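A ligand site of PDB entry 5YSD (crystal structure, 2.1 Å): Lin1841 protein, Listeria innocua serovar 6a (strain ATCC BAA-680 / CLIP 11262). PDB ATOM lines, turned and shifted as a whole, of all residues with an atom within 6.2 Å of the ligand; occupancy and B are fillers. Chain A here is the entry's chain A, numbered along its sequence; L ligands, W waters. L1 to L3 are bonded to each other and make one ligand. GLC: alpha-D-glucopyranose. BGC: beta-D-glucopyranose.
OG1 of Thr 71 sits at hydrogen-bond distance from O4 of BGC L3, 2.7 Å away.
An oxygen (O4) of BGC L2 is in hydrogen-bond range of the side-chain carboxylate of Glu 20.
The backbone NH (N) of Thr 71 lies within hydrogen-bond range of an oxygen (O4) of BGC L3 (3.1 Å).
An oxygen (O3) of BGC L2 sits at hydrogen-bond distance from the side-chain hydroxyl of Tyr 120 (2.6 Å).
An oxygen (O4) of BGC L3 lies within hydrogen-bond range of the backbone NH of Thr 70.
The indole nitrogen (NE1) of Trp 46 lies within hydrogen-bond range of an oxygen (O6) of BGC L2, 3.3 Å away.
An oxygen (O3) of BGC L3 lies within hydrogen-bond range of the side-chain hydroxyl (OG1) of Thr 70 (2.6 Å).
OE2 of Glu 122 lies within hydrogen-bond range of O2 of BGC L3 (2.4 Å).
The backbone carbonyl oxygen (O) of Gly 276 lies close to an oxygen (O3) of BGC L3 (3.4 Å).
O6 of GLC L1 is in hydrogen-bond range of OD2 of Asp 168.
An oxygen (O2) of BGC L3 is in hydrogen-bond range of the backbone NH (N) of Gly 276 (2.9 Å).
OE1 of Gln 172 lies within hydrogen-bond range of O4 of GLC L1 (2.6 Å).
NE of Arg 124 lies within salt-bridge range of OE1 of Glu 122 (2.7 Å).
OD1 of Asp 168 sits at hydrogen-bond distance from N of Asn 170, at 3.0 Å.
The backbone carbonyl oxygen of Gly 276 is in hydrogen-bond range of the backbone NH of Thr 70 (3.1 Å).
OE1 of Glu 171 lies within salt-bridge range of NH1 of Arg 124.
NE1 of Trp 72 lies within hydrogen-bond range of OE1 of Glu 352 (3.0 Å).
The side-chain carboxylate (OE2) of Glu 352 is in hydrogen-bond range of the side-chain amide nitrogen (NE2) of Gln 172 (2.7 Å).
The backbone NH (N) of Ala 277 is in hydrogen-bond range of the backbone carbonyl oxygen (O) of Tyr 120 (2.9 Å).
The backbone NH (N) of Gly 275 is in hydrogen-bond range of the backbone carbonyl oxygen (O) of Glu 122.
CA of Gly 18 touches O6 of BGC L2 (3.5 Å).
Asp 19 touches the ligand.
C of Gly 69 touches O4 of BGC L3 (3.3 Å).
CZ2 of Trp 72 touches C6 of BGC L3, at 3.5 Å.
NH2 of Arg 124 touches O2 of BGC L2, 3.7 Å away.
O of Asn 170 touches C6 of GLC L1, 3.6 Å away.
OE1 of Glu 171 touches C4 of GLC L1, at 3.6 Å.
CD2 of Trp 243 touches C5 of BGC L2 (3.5 Å).
CA of Gly 275 touches O3 of BGC L3, 3.3 Å away.
Hydrophobic or aromatic side chains within 4 Å of the ligand: Trp 46, Trp 72, Tyr 120 and Trp 243.
The nearest printed residue that does not touch the ligand is Glu 352 (4.6 Å).
Water W2 lies within hydrogen-bond range of an oxygen (O6) of BGC L3 (2.6 Å), the side-chain hydroxyl (OG1) of Thr 71 (2.8 Å) and the side-chain carboxylate (OE1) of Glu 352 (2.8 Å).
Water W3 lies within hydrogen-bond range of an oxygen (O4) of BGC L2 (2.7 Å) and the backbone NH of Trp 243 (3.2 Å).
Water W1 lies within hydrogen-bond range of OE2 of Glu 171, NH2 of Arg 124 and O3 of GLC L1.
Water W8 lies within hydrogen-bond range of the side-chain amide nitrogen of Gln 172, the backbone carbonyl oxygen of Trp 46 and an oxygen (O6) of BGC L3.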
ATOM      1  N   MET A  17      12.138  -9.939  30.541  1.00  0.00           N
ATOM      2  CA  MET A  17      10.831  -9.746  31.181  1.00  0.00           C
ATOM      3  C   MET A  17      10.004 -11.013  31.212  1.00  0.00           C
ATOM      4  O   MET A  17      10.123 -11.858  30.351  1.00  0.00           O
ATOM      5  CB  MET A  17      10.004  -8.628  30.494  1.00  0.00           C
ATOM      6  CG  MET A  17      10.623  -7.262  30.523  1.00  0.00           C
ATOM      7  SD  MET A  17      11.626  -7.035  29.060  1.00  0.00           S
ATOM      8  CE  MET A  17      12.489  -5.505  29.457  1.00  0.00           C
ATOM      9  N   GLY A  18       9.127 -11.117  32.202  1.00  0.00           N
ATOM     10  CA  GLY A  18       8.175 -12.204  32.350  1.00  0.00           C
ATOM     11  C   GLY A  18       8.767 -13.566  32.542  1.00  0.00           C
ATOM     12  O   GLY A  18       9.965 -13.714  32.871  1.00  0.00           O
ATOM     13  N   ASP A  19       7.934 -14.577  32.321  1.00  0.00           N
ATOM     14  CA  ASP A  19       8.348 -16.000  32.432  1.00  0.00           C
ATOM     15  C   ASP A  19       9.383 -16.466  31.409  1.00  0.00           C
ATOM     16  O   ASP A  19      10.243 -17.340  31.736  1.00  0.00           O
ATOM     17  CB  ASP A  19       7.149 -16.942  32.479  1.00  0.00           C
ATOM     18  CG  ASP A  19       7.055 -17.630  33.822  1.00  0.00           C
ATOM     19  OD1 ASP A  19       7.041 -16.926  34.861  1.00  0.00           O
ATOM     20  OD2 ASP A  19       7.041 -18.891  33.834  1.00  0.00           O
ATOM     21  N   GLU A  20       9.345 -15.830  30.236  1.00  0.00           N
ATOM     22  CA  GLU A  20      10.288 -16.089  29.177  1.00  0.00           C
ATOM     23  C   GLU A  20      11.747 -15.765  29.567  1.00  0.00           C
ATOM     24  O   GLU A  20      12.696 -16.356  29.023  1.00  0.00           O
ATOM     25  CB  GLU A  20       9.913 -15.298  27.904  1.00  0.00           C
ATOM     26  CG  GLU A  20       8.533 -15.675  27.302  1.00  0.00           C
ATOM     27  CD  GLU A  20       7.322 -14.997  27.962  1.00  0.00           C
ATOM     28  OE1 GLU A  20       7.484 -14.153  28.913  1.00  0.00           O
ATOM     29  OE2 GLU A  20       6.187 -15.319  27.596  1.00  0.00           O
ATOM     30  N   TRP A  46       6.726  -7.098  33.379  1.00  0.00           N
ATOM     31  CA  TRP A  46       6.104  -6.303  32.349  1.00  0.00           C
ATOM     32  C   TRP A  46       5.402  -5.075  32.871  1.00  0.00           C
ATOM     33  O   TRP A  46       5.468  -4.069  32.217  1.00  0.00           O
ATOM     34  CB  TRP A  46       5.090  -7.133  31.526  1.00  0.00           C
ATOM     35  CG  TRP A  46       5.762  -8.078  30.535  1.00  0.00           C
ATOM     36  CD1 TRP A  46       5.839  -9.489  30.604  1.00  0.00           C
ATOM     37  CD2 TRP A  46       6.478  -7.701  29.355  1.00  0.00           C
ATOM     38  NE1 TRP A  46       6.506  -9.953  29.531  1.00  0.00           N
ATOM     39  CE2 TRP A  46       6.928  -8.907  28.742  1.00  0.00           C
ATOM     40  CE3 TRP A  46       6.795  -6.479  28.771  1.00  0.00           C
ATOM     41  CZ2 TRP A  46       7.647  -8.915  27.558  1.00  0.00           C
ATOM     42  CZ3 TRP A  46       7.522  -6.474  27.567  1.00  0.00           C
ATOM     43  CH2 TRP A  46       7.932  -7.672  26.961  1.00  0.00           C
ATOM     44  N   ALA A  47       4.805  -5.115  34.054  1.00  0.00           N
ATOM     45  CA  ALA A  47       4.130  -3.944  34.614  1.00  0.00           C
ATOM     46  C   ALA A  47       5.095  -2.849  35.068  1.00  0.00           C
ATOM     47  O   ALA A  47       4.691  -1.717  35.235  1.00  0.00           O
ATOM     48  CB  ALA A  47       3.207  -4.364  35.729  1.00  0.00           C
ATOM     49  N   GLN A  67      15.463  -6.901  25.935  1.00  0.00           N
ATOM     50  CA  GLN A  67      14.172  -7.438  25.449  1.00  0.00           C
ATOM     51  C   GLN A  67      13.175  -6.281  25.350  1.00  0.00           C
ATOM     52  O   GLN A  67      12.982  -5.530  26.335  1.00  0.00           O
ATOM     53  CB  GLN A  67      13.647  -8.535  26.292  1.00  0.00           C
ATOM     54  CG  GLN A  67      12.403  -9.283  25.795  1.00  0.00           C
ATOM     55  CD  GLN A  67      11.857 -10.247  26.867  1.00  0.00           C
ATOM     56  OE1 GLN A  67      12.618 -10.666  27.731  1.00  0.00           O
ATOM     57  NE2 GLN A  67      10.540 -10.507  26.890  1.00  0.00           N
ATOM     58  N   MET A  68      12.570  -6.139  24.166  1.00  0.00           N
ATOM     59  CA  MET A  68      11.650  -5.086  23.908  1.00  0.00           C
ATOM     60  C   MET A  68      10.285  -5.640  23.570  1.00  0.00           C
ATOM     61  O   MET A  68      10.087  -6.297  22.532  1.00  0.00           O
ATOM     62  CB  MET A  68      12.135  -4.241  22.700  1.00  0.00           C
ATOM     63  CG  MET A  68      13.287  -3.303  22.964  1.00  0.00           C
ATOM     64  SD  MET A  68      12.912  -2.040  24.200  1.00  0.00           S
ATOM     65  CE  MET A  68      11.338  -1.456  23.599  1.00  0.00           C
ATOM     66  N   GLY A  69       9.320  -5.255  24.367  1.00  0.00           N
ATOM     67  CA  GLY A  69       7.903  -5.460  23.941  1.00  0.00           C
ATOM     68  C   GLY A  69       7.620  -4.814  22.633  1.00  0.00           C
ATOM     69  O   GLY A  69       7.979  -3.636  22.425  1.00  0.00           O
ATOM     70  N   THR A  70       6.987  -5.555  21.742  1.00  0.00           N
ATOM     71  CA  THR A  70       6.714  -5.054  20.388  1.00  0.00           C
ATOM     72  C   THR A  70       6.028  -3.679  20.352  1.00  0.00           C
ATOM     73  O   THR A  70       6.329  -2.876  19.484  1.00  0.00           O
ATOM     74  CB  THR A  70       5.906  -6.041  19.557  1.00  0.00           C
ATOM     75  OG1 THR A  70       4.678  -6.338  20.217  1.00  0.00           O
ATOM     76  CG2 THR A  70       6.685  -7.347  19.258  1.00  0.00           C
ATOM     77  N   THR A  71       5.091  -3.437  21.274  1.00  0.00           N
ATOM     78  CA  THR A  71       4.302  -2.192  21.268  1.00  0.00           C
ATOM     79  C   THR A  71       5.134  -0.944  21.651  1.00  0.00           C
ATOM     80  O   THR A  71       4.735   0.159  21.393  1.00  0.00           O
ATOM     81  CB  THR A  71       3.093  -2.247  22.181  1.00  0.00           C
ATOM     82  OG1 THR A  71       3.535  -2.390  23.535  1.00  0.00           O
ATOM     83  CG2 THR A  71       2.156  -3.403  21.785  1.00  0.00           C
ATOM     84  N   TRP A  72       6.279  -1.179  22.308  1.00  0.00           N
ATOM     85  CA  TRP A  72       7.229  -0.143  22.693  1.00  0.00           C
ATOM     86  C   TRP A  72       8.342   0.116  21.703  1.00  0.00           C
ATOM     87  O   TRP A  72       9.081   1.064  21.872  1.00  0.00           O
ATOM     88  CB  TRP A  72       7.798  -0.439  24.058  1.00  0.00           C
ATOM     89  CG  TRP A  72       6.721  -0.591  25.134  1.00  0.00           C
ATOM     90  CD1 TRP A  72       5.452  -0.031  25.117  1.00  0.00           C
ATOM     91  CD2 TRP A  72       6.805  -1.333  26.336  1.00  0.00           C
ATOM     92  NE1 TRP A  72       4.778  -0.367  26.238  1.00  0.00           N
ATOM     93  CE2 TRP A  72       5.574  -1.176  27.011  1.00  0.00           C
ATOM     94  CE3 TRP A  72       7.811  -2.135  26.913  1.00  0.00           C
ATOM     95  CZ2 TRP A  72       5.304  -1.796  28.233  1.00  0.00           C
ATOM     96  CZ3 TRP A  72       7.552  -2.747  28.145  1.00  0.00           C
ATOM     97  CH2 TRP A  72       6.306  -2.583  28.782  1.00  0.00           C
ATOM     98  N   TYR A 120      10.162 -13.755  20.106  1.00  0.00           N
ATOM     99  CA  TYR A 120       8.941 -14.583  20.083  1.00  0.00           C
ATOM    100  C   TYR A 120       7.734 -13.691  19.728  1.00  0.00           C
ATOM    101  O   TYR A 120       7.801 -12.419  19.834  1.00  0.00           O
ATOM    102  CB  TYR A 120       8.719 -15.355  21.426  1.00  0.00           C
ATOM    103  CG  TYR A 120       8.307 -14.520  22.553  1.00  0.00           C
ATOM    104  CD1 TYR A 120       6.950 -14.195  22.772  1.00  0.00           C
ATOM    105  CD2 TYR A 120       9.230 -13.945  23.373  1.00  0.00           C
ATOM    106  CE1 TYR A 120       6.586 -13.322  23.798  1.00  0.00           C
ATOM    107  CE2 TYR A 120       8.858 -13.085  24.418  1.00  0.00           C
ATOM    108  CZ  TYR A 120       7.529 -12.746  24.616  1.00  0.00           C
ATOM    109  OH  TYR A 120       7.149 -11.928  25.665  1.00  0.00           O
ATOM    110  N   GLU A 122       3.216 -13.389  19.829  1.00  0.00           N
ATOM    111  CA  GLU A 122       2.010 -13.924  20.518  1.00  0.00           C
ATOM    112  C   GLU A 122       0.786 -13.254  19.922  1.00  0.00           C
ATOM    113  O   GLU A 122       0.888 -12.194  19.254  1.00  0.00           O
ATOM    114  CB  GLU A 122       2.084 -13.779  22.106  1.00  0.00           C
ATOM    115  CG  GLU A 122       2.341 -12.371  22.621  1.00  0.00           C
ATOM    116  CD  GLU A 122       1.126 -11.480  22.746  1.00  0.00           C
ATOM    117  OE1 GLU A 122       0.006 -11.892  22.497  1.00  0.00           O
ATOM    118  OE2 GLU A 122       1.293 -10.290  23.103  1.00  0.00           O
ATOM    119  N   ARG A 124      -3.751 -13.166  20.909  1.00  0.00           N
ATOM    120  CA  ARG A 124      -4.734 -13.456  21.971  1.00  0.00           C
ATOM    121  C   ARG A 124      -5.923 -14.225  21.423  1.00  0.00           C
ATOM    122  O   ARG A 124      -6.449 -13.911  20.372  1.00  0.00           O
ATOM    123  CB  ARG A 124      -5.241 -12.134  22.558  1.00  0.00           C
ATOM    124  CG  ARG A 124      -4.185 -11.152  22.973  1.00  0.00           C
ATOM    125  CD  ARG A 124      -3.156 -11.803  23.910  1.00  0.00           C
ATOM    126  NE  ARG A 124      -1.993 -11.010  24.137  1.00  0.00           N
ATOM    127  CZ  ARG A 124      -1.829 -10.110  25.118  1.00  0.00           C
ATOM    128  NH1 ARG A 124      -2.798  -9.773  25.958  1.00  0.00           N
ATOM    129  NH2 ARG A 124      -0.686  -9.456  25.202  1.00  0.00           N
ATOM    130  N   ASP A 168      -9.835  -7.762  31.400  1.00  0.00           N
ATOM    131  CA  ASP A 168      -8.684  -7.313  32.152  1.00  0.00           C
ATOM    132  C   ASP A 168      -8.542  -5.784  32.008  1.00  0.00           C
ATOM    133  O   ASP A 168      -8.260  -5.323  30.942  1.00  0.00           O
ATOM    134  CB  ASP A 168      -7.441  -8.062  31.671  1.00  0.00           C
ATOM    135  CG  ASP A 168      -6.186  -7.746  32.501  1.00  0.00           C
ATOM    136  OD1 ASP A 168      -6.211  -6.803  33.327  1.00  0.00           O
ATOM    137  OD2 ASP A 168      -5.145  -8.485  32.299  1.00  0.00           O
ATOM    138  N   ASN A 170      -6.300  -3.783  32.931  1.00  0.00           N
ATOM    139  CA  ASN A 170      -4.926  -3.392  32.740  1.00  0.00           C
ATOM    140  C   ASN A 170      -4.304  -3.886  31.422  1.00  0.00           C
ATOM    141  O   ASN A 170      -3.128  -3.594  31.135  1.00  0.00           O
ATOM    142  CB  ASN A 170      -4.083  -3.858  33.882  1.00  0.00           C
ATOM    143  CG  ASN A 170      -4.502  -3.284  35.231  1.00  0.00           C
ATOM    144  OD1 ASN A 170      -4.618  -4.044  36.156  1.00  0.00           O
ATOM    145  ND2 ASN A 170      -4.687  -1.989  35.349  1.00  0.00           N
ATOM    146  N   GLU A 171      -5.080  -4.603  30.613  1.00  0.00           N
ATOM    147  CA  GLU A 171      -4.628  -5.146  29.388  1.00  0.00           C
ATOM    148  C   GLU A 171      -4.720  -4.081  28.314  1.00  0.00           C
ATOM    149  O   GLU A 171      -5.806  -3.740  27.871  1.00  0.00           O
ATOM    150  CB  GLU A 171      -5.473  -6.371  28.990  1.00  0.00           C
ATOM    151  CG  GLU A 171      -5.098  -6.938  27.596  1.00  0.00           C
ATOM    152  CD  GLU A 171      -3.616  -7.181  27.449  1.00  0.00           C
ATOM    153  OE1 GLU A 171      -3.076  -7.908  28.306  1.00  0.00           O
ATOM    154  OE2 GLU A 171      -2.970  -6.645  26.518  1.00  0.00           O
ATOM    155  N   GLN A 172      -3.590  -3.672  27.816  1.00  0.00           N
ATOM    156  CA  GLN A 172      -3.537  -2.602  26.788  1.00  0.00           C
ATOM    157  C   GLN A 172      -4.238  -2.938  25.483  1.00  0.00           C
ATOM    158  O   GLN A 172      -4.770  -2.094  24.829  1.00  0.00           O
ATOM    159  CB  GLN A 172      -2.048  -2.208  26.533  1.00  0.00           C
ATOM    160  CG  GLN A 172      -1.291  -1.687  27.771  1.00  0.00           C
ATOM    161  CD  GLN A 172      -0.445  -2.716  28.471  1.00  0.00           C
ATOM    162  OE1 GLN A 172      -0.804  -3.911  28.482  1.00  0.00           O
ATOM    163  NE2 GLN A 172       0.727  -2.285  29.034  1.00  0.00           N
ATOM    164  N   PRO A 242      -0.384 -17.402  24.648  1.00  0.00           N
ATOM    165  CA  PRO A 242       0.326 -18.681  24.841  1.00  0.00           C
ATOM    166  C   PRO A 242       0.797 -18.944  26.243  1.00  0.00           C
ATOM    167  O   PRO A 242       0.684 -20.087  26.685  1.00  0.00           O
ATOM    168  CB  PRO A 242       1.485 -18.622  23.842  1.00  0.00           C
ATOM    169  CG  PRO A 242       0.944 -17.781  22.730  1.00  0.00           C
ATOM    170  CD  PRO A 242       0.136 -16.708  23.431  1.00  0.00           C
ATOM    171  N   TRP A 243       1.376 -17.932  26.911  1.00  0.00           N
ATOM    172  CA  TRP A 243       1.810 -18.089  28.284  1.00  0.00           C
ATOM    173  C   TRP A 243       0.727 -18.665  29.166  1.00  0.00           C
ATOM    174  O   TRP A 243       1.041 -19.422  30.064  1.00  0.00           O
ATOM    175  CB  TRP A 243       2.401 -16.828  28.860  1.00  0.00           C
ATOM    176  CG  TRP A 243       1.390 -15.802  29.342  1.00  0.00           C
ATOM    177  CD1 TRP A 243       0.926 -15.613  30.620  1.00  0.00           C
ATOM    178  CD2 TRP A 243       0.704 -14.801  28.528  1.00  0.00           C
ATOM    179  NE1 TRP A 243       0.036 -14.577  30.641  1.00  0.00           N
ATOM    180  CE2 TRP A 243      -0.096 -14.041  29.400  1.00  0.00           C
ATOM    181  CE3 TRP A 243       0.770 -14.450  27.192  1.00  0.00           C
ATOM    182  CZ2 TRP A 243      -0.854 -12.965  28.964  1.00  0.00           C
ATOM    183  CZ3 TRP A 243      -0.001 -13.360  26.739  1.00  0.00           C
ATOM    184  CH2 TRP A 243      -0.806 -12.655  27.633  1.00  0.00           C
ATOM    185  N   LEU A 274      -1.267  -8.757  17.457  1.00  0.00           N
ATOM    186  CA  LEU A 274       0.034  -9.413  17.270  1.00  0.00           C
ATOM    187  C   LEU A 274       1.028  -8.674  18.151  1.00  0.00           C
ATOM    188  O   LEU A 274       1.262  -7.410  18.022  1.00  0.00           O
ATOM    189  CB  LEU A 274       0.494  -9.430  15.817  1.00  0.00           C
ATOM    190  CG  LEU A 274       1.823 -10.216  15.565  1.00  0.00           C
ATOM    191  CD1 LEU A 274       1.626 -11.768  15.661  1.00  0.00           C
ATOM    192  CD2 LEU A 274       2.456  -9.899  14.251  1.00  0.00           C
ATOM    193  N   GLY A 275       1.608  -9.462  19.074  1.00  0.00           N
ATOM    194  CA  GLY A 275       2.641  -8.987  19.957  1.00  0.00           C
ATOM    195  C   GLY A 275       3.831  -9.906  20.054  1.00  0.00           C
ATOM    196  O   GLY A 275       4.142 -10.667  19.135  1.00  0.00           O
ATOM    197  N   GLY A 276       4.476  -9.821  21.221  1.00  0.00           N
ATOM    198  CA  GLY A 276       5.618 -10.641  21.555  1.00  0.00           C
ATOM    199  C   GLY A 276       6.746  -9.693  21.884  1.00  0.00           C
ATOM    200  O   GLY A 276       6.515  -8.589  22.342  1.00  0.00           O
ATOM    201  N   ALA A 277       7.968 -10.135  21.682  1.00  0.00           N
ATOM    202  CA  ALA A 277       9.158  -9.294  21.986  1.00  0.00           C
ATOM    203  C   ALA A 277      10.255  -9.522  21.058  1.00  0.00           C
ATOM    204  O   ALA A 277      10.357 -10.581  20.438  1.00  0.00           O
ATOM    205  CB  ALA A 277       9.674  -9.572  23.421  1.00  0.00           C
ATOM    206  N   GLU A 352       1.978   3.486  24.380  1.00  0.00           N
ATOM    207  CA  GLU A 352       1.749   3.128  25.795  1.00  0.00           C
ATOM    208  C   GLU A 352       0.969   4.171  26.560  1.00  0.00           C
ATOM    209  O   GLU A 352       0.131   3.836  27.363  1.00  0.00           O
ATOM    210  CB  GLU A 352       3.000   2.776  26.553  1.00  0.00           C
ATOM    211  CG  GLU A 352       2.794   2.116  27.893  1.00  0.00           C
ATOM    212  CD  GLU A 352       2.031   0.764  27.832  1.00  0.00           C
ATOM    213  OE1 GLU A 352       1.915   0.149  26.731  1.00  0.00           O
ATOM    214  OE2 GLU A 352       1.567   0.319  28.901  1.00  0.00           O
HETATM  215  C1  GLC L   1       0.263  -9.588  30.747  1.00  0.00           C
HETATM  216  C2  GLC L   1       0.991  -8.852  29.606  1.00  0.00           C
HETATM  217  C3  GLC L   1       1.054  -7.359  29.841  1.00  0.00           C
HETATM  218  C4  GLC L   1      -0.288  -6.808  30.280  1.00  0.00           C
HETATM  219  C5  GLC L   1      -0.834  -7.518  31.527  1.00  0.00           C
HETATM  220  C6  GLC L   1      -2.221  -6.963  31.819  1.00  0.00           C
HETATM  221  O1  GLC L   1       1.172  -9.689  31.780  1.00  0.00           O
HETATM  222  O2  GLC L   1       2.376  -9.247  29.443  1.00  0.00           O
HETATM  223  O3  GLC L   1       1.431  -6.819  28.563  1.00  0.00           O
HETATM  224  O4  GLC L   1      -0.113  -5.402  30.499  1.00  0.00           O
HETATM  225  O5  GLC L   1      -0.884  -8.939  31.343  1.00  0.00           O
HETATM  226  O6  GLC L   1      -2.836  -7.712  32.874  1.00  0.00           O
HETATM  227  C2  BGC L   2       3.433 -10.195  27.439  1.00  0.00           C
HETATM  228  C3  BGC L   2       3.717 -11.467  26.661  1.00  0.00           C
HETATM  229  C4  BGC L   2       4.308 -12.531  27.597  1.00  0.00           C
HETATM  230  C5  BGC L   2       3.496 -12.706  28.894  1.00  0.00           C
HETATM  231  C6  BGC L   2       4.202 -13.612  29.926  1.00  0.00           C
HETATM  232  C1  BGC L   2       2.559 -10.454  28.688  1.00  0.00           C
HETATM  233  O2  BGC L   2       2.746  -9.280  26.590  1.00  0.00           O
HETATM  234  O3  BGC L   2       4.617 -11.242  25.556  1.00  0.00           O
HETATM  235  O4  BGC L   2       4.311 -13.732  26.853  1.00  0.00           O
HETATM  236  O5  BGC L   2       3.195 -11.417  29.514  1.00  0.00           O
HETATM  237  O6  BGC L   2       5.472 -13.043  30.227  1.00  0.00           O
HETATM  238  C2  BGC L   3       3.144  -8.154  24.562  1.00  0.00           C
HETATM  239  C3  BGC L   3       3.913  -7.062  23.834  1.00  0.00           C
HETATM  240  C4  BGC L   3       3.762  -5.781  24.629  1.00  0.00           C
HETATM  241  C5  BGC L   3       4.150  -6.029  26.115  1.00  0.00           C
HETATM  242  C6  BGC L   3       4.001  -4.770  26.927  1.00  0.00           C
HETATM  243  C1  BGC L   3       3.577  -8.295  26.020  1.00  0.00           C
HETATM  244  O2  BGC L   3       3.400  -9.388  23.916  1.00  0.00           O
HETATM  245  O3  BGC L   3       3.489  -6.952  22.441  1.00  0.00           O
HETATM  246  O4  BGC L   3       4.650  -4.850  24.023  1.00  0.00           O
HETATM  247  O5  BGC L   3       3.388  -7.090  26.725  1.00  0.00           O
HETATM  248  O6  BGC L   3       2.622  -4.388  27.045  1.00  0.00           O
HETATM  249  O   HOH W   1      -0.532  -6.772  26.313  1.00  0.00           O
HETATM  250  O   HOH W   2       1.694  -2.402  25.609  1.00  0.00           O
HETATM  251  O   HOH W   3       3.152 -15.729  25.420  1.00  0.00           O
HETATM  252  O   HOH W   4       1.452  -4.771  32.541  1.00  0.00           O
HETATM  253  O   HOH W   5       3.409 -11.063  32.203  1.00  0.00           O
HETATM  254  O   HOH W   6       1.801  -7.259  33.948  1.00  0.00           O
HETATM  255  O   HOH W   7      -2.318  -7.162  35.460  1.00  0.00           O
HETATM  256  O   HOH W   8       2.909  -4.185  30.272  1.00  0.00           O
HETATM  257  O   HOH W   9       0.592  -6.412  22.257  1.00  0.00           O
